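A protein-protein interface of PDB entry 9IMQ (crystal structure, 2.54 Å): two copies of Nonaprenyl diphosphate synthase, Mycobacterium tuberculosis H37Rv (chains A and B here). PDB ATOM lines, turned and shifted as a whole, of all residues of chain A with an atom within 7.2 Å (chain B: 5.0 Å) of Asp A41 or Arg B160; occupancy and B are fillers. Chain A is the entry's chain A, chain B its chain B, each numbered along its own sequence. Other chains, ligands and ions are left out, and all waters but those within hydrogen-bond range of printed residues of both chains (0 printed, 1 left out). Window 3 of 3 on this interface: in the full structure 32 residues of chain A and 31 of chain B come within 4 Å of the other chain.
No position is printed for both chains.
Hydrophobic or aromatic side chains of chain A within 4 Å of the printed part of chain B: Val A43, Met A44, Leu A123 and Tyr A127.
Hydrophobic or aromatic side chains of chain B within 4 Å of the printed part of chain A: Met B159.
Among the printed residues, Asp or Glu carboxylates within 4 Å of a Lys or Arg side-chain nitrogen of the other chain: Asp A41 with Arg B160.
The backbone carbonyl oxygen (O) of Val A43 is in hydrogen-bond range of the guanidinium group (NH1) of Arg B163.
NH2 of Arg B160 is in salt-bridge range of OD2 of Asp A41, 2.6 Å away.
CG2 of Thr B156 touches CB of Asp A41, 3.8 Å away.
O of Val A43 touches CG of Met B159 (3.5 Å).
Arg B160 touches Val A43.
Met A44 touches Met B159 (CE to CE, 3.5 Å).
Gln B158 touches Leu A123.
Met B159 touches Leu A123 (CE to CB, 3.8 Å).
CE2 of Tyr A127 touches OG1 of Thr B156, at 3.4 Å.
NH1 of Arg B160 sits at hydrogen-bond distance from OE1 of Gln B174, at 3.2 Å.
The guanidinium group (NE) of Arg B160 is in salt-bridge range of the side-chain carboxylate (OE1) of Glu B181, 2.9 Å away.
N of Val A43 sits close to OD1 of Asp A41, at 3.2 Å.
The backbone carbonyl oxygen (O) of Gln B158 is in hydrogen-bond range of the side-chain hydroxyl (OG1) of Thr B162.
Asp A41 touches just these residues of chain B: Thr B156 (3.8 Å) and Arg B160 (2.6 Å).
Printed residues of chain A within 4 Å of Gln B158: Leu A123 (3.8 Å).
Of the printed residues of chain A, Met B159 touches Val A43 (3.5 Å), Met A44 (3.5 Å) and Leu A123 (3.8 Å).
Of chain A, only Asp A41 (2.6 Å) and Val A43 (3.9 Å) come within 4 Å of Arg B160.
The nearest printed residue of chain B that does not touch Asp A41 is Lys B177 (4.4 Å).
The nearest residue of chain A that does not touch Arg B160 is Glu A42 (6.0 Å).
The nearest printed residue of chain A that does not touch Arg B163 is Asp A46 (4.02 Å).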
ATOM      1  N   LEU A  37      -3.953 -32.643  -1.732  1.00  0.00           N
ATOM      2  CA  LEU A  37      -5.103 -31.761  -1.554  1.00  0.00           C
ATOM      3  C   LEU A  37      -4.707 -30.475  -0.840  1.00  0.00           C
ATOM      4  O   LEU A  37      -5.138 -29.379  -1.228  1.00  0.00           O
ATOM      5  CB  LEU A  37      -6.209 -32.468  -0.766  1.00  0.00           C
ATOM      6  CG  LEU A  37      -6.718 -33.785  -1.346  1.00  0.00           C
ATOM      7  CD1 LEU A  37      -7.772 -34.416  -0.423  1.00  0.00           C
ATOM      8  CD2 LEU A  37      -7.243 -33.577  -2.756  1.00  0.00           C
ATOM      9  N   ARG A  38      -3.899 -30.593   0.218  1.00  0.00           N
ATOM     10  CA  ARG A  38      -3.588 -29.432   1.043  1.00  0.00           C
ATOM     11  C   ARG A  38      -2.847 -28.373   0.238  1.00  0.00           C
ATOM     12  O   ARG A  38      -2.970 -27.182   0.526  1.00  0.00           O
ATOM     13  CB  ARG A  38      -2.775 -29.860   2.267  1.00  0.00           C
ATOM     14  CG  ARG A  38      -3.624 -30.261   3.472  1.00  0.00           C
ATOM     15  CD  ARG A  38      -4.602 -29.148   3.831  1.00  0.00           C
ATOM     16  NE  ARG A  38      -5.269 -29.300   5.126  1.00  0.00           N
ATOM     17  CZ  ARG A  38      -4.663 -29.508   6.292  1.00  0.00           C
ATOM     18  NH1 ARG A  38      -3.344 -29.597   6.387  1.00  0.00           N
ATOM     19  NH2 ARG A  38      -5.399 -29.604   7.398  1.00  0.00           N
ATOM     20  N   GLN A  39      -2.121 -28.791  -0.798  1.00  0.00           N
ATOM     21  CA  GLN A  39      -1.357 -27.896  -1.647  1.00  0.00           C
ATOM     22  C   GLN A  39      -2.244 -27.049  -2.554  1.00  0.00           C
ATOM     23  O   GLN A  39      -1.750 -26.084  -3.148  1.00  0.00           O
ATOM     24  CB  GLN A  39      -0.338 -28.755  -2.421  1.00  0.00           C
ATOM     25  CG  GLN A  39       0.010 -28.385  -3.855  1.00  0.00           C
ATOM     26  CD  GLN A  39       1.064 -29.322  -4.446  1.00  0.00           C
ATOM     27  OE1 GLN A  39       1.625 -30.168  -3.741  1.00  0.00           O
ATOM     28  NE2 GLN A  39       1.331 -29.176  -5.742  1.00  0.00           N
ATOM     29  N   ALA A  40      -3.543 -27.346  -2.623  1.00  0.00           N
ATOM     30  CA  ALA A  40      -4.470 -26.602  -3.465  1.00  0.00           C
ATOM     31  C   ALA A  40      -4.622 -25.164  -2.988  1.00  0.00           C
ATOM     32  O   ALA A  40      -4.366 -24.832  -1.827  1.00  0.00           O
ATOM     33  CB  ALA A  40      -5.845 -27.263  -3.484  1.00  0.00           C
ATOM     34  N   ASP A  41      -5.058 -24.304  -3.909  1.00  0.00           N
ATOM     35  CA  ASP A  41      -5.305 -22.909  -3.577  1.00  0.00           C
ATOM     36  C   ASP A  41      -6.269 -22.823  -2.403  1.00  0.00           C
ATOM     37  O   ASP A  41      -7.205 -23.619  -2.296  1.00  0.00           O
ATOM     38  CB  ASP A  41      -5.873 -22.173  -4.792  1.00  0.00           C
ATOM     39  CG  ASP A  41      -5.960 -20.665  -4.587  1.00  0.00           C
ATOM     40  OD1 ASP A  41      -6.822 -20.199  -3.814  1.00  0.00           O
ATOM     41  OD2 ASP A  41      -5.188 -19.929  -5.235  1.00  0.00           O
ATOM     42  N   GLU A  42      -6.005 -21.863  -1.512  1.00  0.00           N
ATOM     43  CA  GLU A  42      -6.793 -21.558  -0.319  1.00  0.00           C
ATOM     44  C   GLU A  42      -8.287 -21.788  -0.503  1.00  0.00           C
ATOM     45  O   GLU A  42      -8.946 -22.335   0.390  1.00  0.00           O
ATOM     46  CB  GLU A  42      -6.565 -20.098   0.094  1.00  0.00           C
ATOM     47  CG  GLU A  42      -6.655 -19.818   1.585  1.00  0.00           C
ATOM     48  CD  GLU A  42      -5.606 -18.805   2.070  1.00  0.00           C
ATOM     49  OE1 GLU A  42      -4.950 -18.152   1.215  1.00  0.00           O
ATOM     50  OE2 GLU A  42      -5.434 -18.673   3.310  1.00  0.00           O
ATOM     51  N   VAL A  43      -8.825 -21.391  -1.662  1.00  0.00           N
ATOM     52  CA  VAL A  43     -10.276 -21.354  -1.842  1.00  0.00           C
ATOM     53  C   VAL A  43     -10.879 -22.734  -1.990  1.00  0.00           C
ATOM     54  O   VAL A  43     -12.091 -22.888  -1.817  1.00  0.00           O
ATOM     55  CB  VAL A  43     -10.675 -20.487  -3.048  1.00  0.00           C
ATOM     56  CG1 VAL A  43     -10.297 -21.177  -4.351  1.00  0.00           C
ATOM     57  CG2 VAL A  43     -12.169 -20.206  -3.015  1.00  0.00           C
ATOM     58  N   MET A  44     -10.077 -23.754  -2.295  1.00  0.00           N
ATOM     59  CA  MET A  44     -10.618 -25.107  -2.370  1.00  0.00           C
ATOM     60  C   MET A  44     -10.667 -25.824  -1.021  1.00  0.00           C
ATOM     61  O   MET A  44     -11.481 -26.738  -0.859  1.00  0.00           O
ATOM     62  CB  MET A  44      -9.808 -25.940  -3.371  1.00  0.00           C
ATOM     63  CG  MET A  44      -9.642 -25.302  -4.733  1.00  0.00           C
ATOM     64  SD  MET A  44     -11.196 -25.343  -5.676  1.00  0.00           S
ATOM     65  CE  MET A  44     -11.690 -27.076  -5.473  1.00  0.00           C
ATOM     66  N   SER A  45      -9.866 -25.387  -0.043  1.00  0.00           N
ATOM     67  CA  SER A  45      -9.474 -26.254   1.072  1.00  0.00           C
ATOM     68  C   SER A  45     -10.669 -26.725   1.895  1.00  0.00           C
ATOM     69  O   SER A  45     -10.702 -27.879   2.335  1.00  0.00           O
ATOM     70  CB  SER A  45      -8.450 -25.537   1.957  1.00  0.00           C
ATOM     71  OG  SER A  45      -7.175 -25.497   1.321  1.00  0.00           O
ATOM     72  N   ASP A  46     -11.658 -25.861   2.108  1.00  0.00           N
ATOM     73  CA  ASP A  46     -12.883 -26.274   2.780  1.00  0.00           C
ATOM     74  C   ASP A  46     -13.477 -27.501   2.101  1.00  0.00           C
ATOM     75  O   ASP A  46     -13.453 -28.607   2.657  1.00  0.00           O
ATOM     76  CB  ASP A  46     -13.916 -25.147   2.774  1.00  0.00           C
ATOM     77  CG  ASP A  46     -13.663 -24.112   3.858  1.00  0.00           C
ATOM     78  OD1 ASP A  46     -12.825 -24.372   4.757  1.00  0.00           O
ATOM     79  OD2 ASP A  46     -14.291 -23.031   3.797  1.00  0.00           O
ATOM     80  N   LEU A  48     -12.485 -29.319  -0.281  1.00  0.00           N
ATOM     81  CA  LEU A  48     -11.576 -30.367  -0.731  1.00  0.00           C
ATOM     82  C   LEU A  48     -11.367 -31.424   0.342  1.00  0.00           C
ATOM     83  O   LEU A  48     -11.423 -32.624   0.061  1.00  0.00           O
ATOM     84  CB  LEU A  48     -10.240 -29.752  -1.139  1.00  0.00           C
ATOM     85  CG  LEU A  48      -9.932 -29.822  -2.626  1.00  0.00           C
ATOM     86  CD1 LEU A  48      -8.483 -29.509  -2.831  1.00  0.00           C
ATOM     87  CD2 LEU A  48     -10.275 -31.196  -3.209  1.00  0.00           C
ATOM     88  N   LEU A 123     -17.721 -28.920  -8.030  1.00  0.00           N
ATOM     89  CA  LEU A 123     -16.390 -28.430  -8.359  1.00  0.00           C
ATOM     90  C   LEU A 123     -15.318 -29.157  -7.558  1.00  0.00           C
ATOM     91  O   LEU A 123     -14.276 -29.548  -8.100  1.00  0.00           O
ATOM     92  CB  LEU A 123     -16.336 -26.929  -8.121  1.00  0.00           C
ATOM     93  CG  LEU A 123     -17.259 -26.110  -9.026  1.00  0.00           C
ATOM     94  CD1 LEU A 123     -17.271 -24.621  -8.628  1.00  0.00           C
ATOM     95  CD2 LEU A 123     -16.915 -26.301 -10.518  1.00  0.00           C
ATOM     96  N   TYR A 127     -12.125 -31.099  -8.950  1.00  0.00           N
ATOM     97  CA  TYR A 127     -10.736 -30.834  -8.598  1.00  0.00           C
ATOM     98  C   TYR A 127     -10.026 -32.111  -8.171  1.00  0.00           C
ATOM     99  O   TYR A 127      -8.805 -32.237  -8.342  1.00  0.00           O
ATOM    100  CB  TYR A 127     -10.680 -29.778  -7.492  1.00  0.00           C
ATOM    101  CG  TYR A 127      -9.295 -29.249  -7.281  1.00  0.00           C
ATOM    102  CD1 TYR A 127      -8.396 -29.912  -6.450  1.00  0.00           C
ATOM    103  CD2 TYR A 127      -8.865 -28.099  -7.933  1.00  0.00           C
ATOM    104  CE1 TYR A 127      -7.105 -29.430  -6.268  1.00  0.00           C
ATOM    105  CE2 TYR A 127      -7.589 -27.617  -7.752  1.00  0.00           C
ATOM    106  CZ  TYR A 127      -6.714 -28.286  -6.925  1.00  0.00           C
ATOM    107  OH  TYR A 127      -5.439 -27.804  -6.756  1.00  0.00           O
ATOM    108  N   THR B 156     -10.438 -24.091  -9.996  1.00  0.00           N
ATOM    109  CA  THR B 156     -10.085 -23.113  -8.976  1.00  0.00           C
ATOM    110  C   THR B 156     -10.698 -21.758  -9.307  1.00  0.00           C
ATOM    111  O   THR B 156     -11.299 -21.107  -8.445  1.00  0.00           O
ATOM    112  CB  THR B 156      -8.563 -23.010  -8.856  1.00  0.00           C
ATOM    113  OG1 THR B 156      -8.013 -24.299  -8.549  1.00  0.00           O
ATOM    114  CG2 THR B 156      -8.178 -22.024  -7.779  1.00  0.00           C
ATOM    115  N   GLY B 157     -10.587 -21.337 -10.569  1.00  0.00           N
ATOM    116  CA  GLY B 157     -11.239 -20.107 -10.985  1.00  0.00           C
ATOM    117  C   GLY B 157     -12.720 -20.095 -10.677  1.00  0.00           C
ATOM    118  O   GLY B 157     -13.268 -19.081 -10.234  1.00  0.00           O
ATOM    119  N   GLN B 158     -13.389 -21.226 -10.894  1.00  0.00           N
ATOM    120  CA  GLN B 158     -14.823 -21.294 -10.645  1.00  0.00           C
ATOM    121  C   GLN B 158     -15.140 -21.199  -9.158  1.00  0.00           C
ATOM    122  O   GLN B 158     -16.126 -20.573  -8.769  1.00  0.00           O
ATOM    123  CB  GLN B 158     -15.383 -22.584 -11.235  1.00  0.00           C
ATOM    124  CG  GLN B 158     -15.308 -22.617 -12.729  1.00  0.00           C
ATOM    125  CD  GLN B 158     -15.818 -23.915 -13.313  1.00  0.00           C
ATOM    126  OE1 GLN B 158     -15.056 -24.876 -13.530  1.00  0.00           O
ATOM    127  NE2 GLN B 158     -17.121 -23.946 -13.591  1.00  0.00           N
ATOM    128  N   MET B 159     -14.323 -21.824  -8.313  1.00  0.00           N
ATOM    129  CA  MET B 159     -14.546 -21.727  -6.876  1.00  0.00           C
ATOM    130  C   MET B 159     -14.374 -20.292  -6.399  1.00  0.00           C
ATOM    131  O   MET B 159     -15.251 -19.742  -5.720  1.00  0.00           O
ATOM    132  CB  MET B 159     -13.592 -22.663  -6.127  1.00  0.00           C
ATOM    133  CG  MET B 159     -14.018 -22.913  -4.683  1.00  0.00           C
ATOM    134  SD  MET B 159     -15.503 -23.923  -4.636  1.00  0.00           S
ATOM    135  CE  MET B 159     -14.827 -25.563  -4.857  1.00  0.00           C
ATOM    136  N   ARG B 160     -13.231 -19.681  -6.734  1.00  0.00           N
ATOM    137  CA  ARG B 160     -13.007 -18.264  -6.463  1.00  0.00           C
ATOM    138  C   ARG B 160     -14.223 -17.439  -6.859  1.00  0.00           C
ATOM    139  O   ARG B 160     -14.803 -16.729  -6.033  1.00  0.00           O
ATOM    140  CB  ARG B 160     -11.763 -17.797  -7.222  1.00  0.00           C
ATOM    141  CG  ARG B 160     -11.140 -16.533  -6.697  1.00  0.00           C
ATOM    142  CD  ARG B 160      -9.802 -16.284  -7.360  1.00  0.00           C
ATOM    143  NE  ARG B 160      -8.871 -17.408  -7.263  1.00  0.00           N
ATOM    144  CZ  ARG B 160      -7.933 -17.525  -6.336  1.00  0.00           C
ATOM    145  NH1 ARG B 160      -7.844 -16.672  -5.330  1.00  0.00           N
ATOM    146  NH2 ARG B 160      -7.052 -18.513  -6.424  1.00  0.00           N
ATOM    147  N   GLU B 161     -14.635 -17.553  -8.122  1.00  0.00           N
ATOM    148  CA  GLU B 161     -15.848 -16.899  -8.603  1.00  0.00           C
ATOM    149  C   GLU B 161     -17.045 -17.179  -7.698  1.00  0.00           C
ATOM    150  O   GLU B 161     -17.614 -16.260  -7.089  1.00  0.00           O
ATOM    151  CB  GLU B 161     -16.153 -17.361 -10.028  1.00  0.00           C
ATOM    152  CG  GLU B 161     -17.486 -16.864 -10.497  1.00  0.00           C
ATOM    153  CD  GLU B 161     -17.521 -16.579 -11.972  1.00  0.00           C
ATOM    154  OE1 GLU B 161     -16.447 -16.579 -12.604  1.00  0.00           O
ATOM    155  OE2 GLU B 161     -18.629 -16.332 -12.501  1.00  0.00           O
ATOM    156  N   THR B 162     -17.442 -18.460  -7.617  1.00  0.00           N
ATOM    157  CA  THR B 162     -18.622 -18.855  -6.852  1.00  0.00           C
ATOM    158  C   THR B 162     -18.564 -18.334  -5.428  1.00  0.00           C
ATOM    159  O   THR B 162     -19.582 -17.919  -4.871  1.00  0.00           O
ATOM    160  CB  THR B 162     -18.753 -20.378  -6.848  1.00  0.00           C
ATOM    161  OG1 THR B 162     -19.269 -20.813  -8.111  1.00  0.00           O
ATOM    162  CG2 THR B 162     -19.672 -20.837  -5.728  1.00  0.00           C
ATOM    163  N   ARG B 163     -17.370 -18.317  -4.840  1.00  0.00           N
ATOM    164  CA  ARG B 163     -17.196 -17.930  -3.448  1.00  0.00           C
ATOM    165  C   ARG B 163     -16.910 -16.445  -3.270  1.00  0.00           C
ATOM    166  O   ARG B 163     -17.236 -15.884  -2.217  1.00  0.00           O
ATOM    167  CB  ARG B 163     -16.084 -18.772  -2.818  1.00  0.00           C
ATOM    168  CG  ARG B 163     -16.407 -20.263  -2.860  1.00  0.00           C
ATOM    169  CD  ARG B 163     -16.373 -20.880  -1.478  1.00  0.00           C
ATOM    170  NE  ARG B 163     -15.120 -20.591  -0.791  1.00  0.00           N
ATOM    171  CZ  ARG B 163     -14.286 -21.517  -0.339  1.00  0.00           C
ATOM    172  NH1 ARG B 163     -14.572 -22.809  -0.427  1.00  0.00           N
ATOM    173  NH2 ARG B 163     -13.141 -21.138   0.218  1.00  0.00           N
ATOM    174  N   GLY B 164     -16.317 -15.785  -4.266  1.00  0.00           N
ATOM    175  CA  GLY B 164     -16.282 -14.332  -4.239  1.00  0.00           C
ATOM    176  C   GLY B 164     -17.668 -13.729  -4.310  1.00  0.00           C
ATOM    177  O   GLY B 164     -17.915 -12.660  -3.744  1.00  0.00           O
ATOM    178  N   THR B 165     -18.592 -14.416  -4.986  1.00  0.00           N
ATOM    179  CA  THR B 165     -19.970 -13.946  -5.086  1.00  0.00           C
ATOM    180  C   THR B 165     -20.709 -14.097  -3.764  1.00  0.00           C
ATOM    181  O   THR B 165     -21.416 -13.179  -3.336  1.00  0.00           O
ATOM    182  CB  THR B 165     -20.698 -14.713  -6.191  1.00  0.00           C
ATOM    183  OG1 THR B 165     -20.499 -14.046  -7.442  1.00  0.00           O
ATOM    184  CG2 THR B 165     -22.193 -14.840  -5.891  1.00  0.00           C
ATOM    185  N   GLN B 174      -9.368 -10.134  -7.292  1.00  0.00           N
ATOM    186  CA  GLN B 174      -9.939 -11.476  -7.322  1.00  0.00           C
ATOM    187  C   GLN B 174     -10.578 -11.754  -8.671  1.00  0.00           C
ATOM    188  O   GLN B 174     -10.512 -12.882  -9.165  1.00  0.00           O
ATOM    189  CB  GLN B 174     -10.950 -11.673  -6.196  1.00  0.00           C
ATOM    190  CG  GLN B 174     -10.310 -11.850  -4.827  1.00  0.00           C
ATOM    191  CD  GLN B 174      -9.322 -13.014  -4.743  1.00  0.00           C
ATOM    192  OE1 GLN B 174      -9.714 -14.169  -4.594  1.00  0.00           O
ATOM    193  NE2 GLN B 174      -8.034 -12.701  -4.804  1.00  0.00           N
ATOM    194  N   LYS B 177      -7.880 -12.486 -11.279  1.00  0.00           N
ATOM    195  CA  LYS B 177      -7.421 -13.841 -11.017  1.00  0.00           C
ATOM    196  C   LYS B 177      -8.460 -14.857 -11.472  1.00  0.00           C
ATOM    197  O   LYS B 177      -8.114 -15.925 -11.994  1.00  0.00           O
ATOM    198  CB  LYS B 177      -7.116 -13.998  -9.530  1.00  0.00           C
ATOM    199  CG  LYS B 177      -5.638 -14.055  -9.177  1.00  0.00           C
ATOM    200  CD  LYS B 177      -5.418 -13.771  -7.684  1.00  0.00           C
ATOM    201  CE  LYS B 177      -5.476 -15.051  -6.842  1.00  0.00           C
ATOM    202  NZ  LYS B 177      -4.434 -16.061  -7.208  1.00  0.00           N
ATOM    203  N   VAL B 178      -9.738 -14.521 -11.317  1.00  0.00           N
ATOM    204  CA  VAL B 178     -10.793 -15.441 -11.707  1.00  0.00           C
ATOM    205  C   VAL B 178     -10.679 -15.777 -13.187  1.00  0.00           C
ATOM    206  O   VAL B 178     -10.616 -16.952 -13.572  1.00  0.00           O
ATOM    207  CB  VAL B 178     -12.175 -14.863 -11.362  1.00  0.00           C
ATOM    208  CG1 VAL B 178     -13.255 -15.573 -12.187  1.00  0.00           C
ATOM    209  CG2 VAL B 178     -12.473 -15.019  -9.874  1.00  0.00           C
ATOM    210  N   GLU B 181      -7.758 -17.828 -14.377  1.00  0.00           N
ATOM    211  CA  GLU B 181      -7.907 -19.223 -13.980  1.00  0.00           C
ATOM    212  C   GLU B 181      -9.046 -19.896 -14.726  1.00  0.00           C
ATOM    213  O   GLU B 181      -8.866 -20.966 -15.320  1.00  0.00           O
ATOM    214  CB  GLU B 181      -8.171 -19.318 -12.486  1.00  0.00           C
ATOM    215  CG  GLU B 181      -6.973 -19.065 -11.651  1.00  0.00           C
ATOM    216  CD  GLU B 181      -7.358 -18.820 -10.223  1.00  0.00           C
ATOM    217  OE1 GLU B 181      -8.545 -18.497  -9.973  1.00  0.00           O
ATOM    218  OE2 GLU B 181      -6.472 -18.967  -9.357  1.00  0.00           O
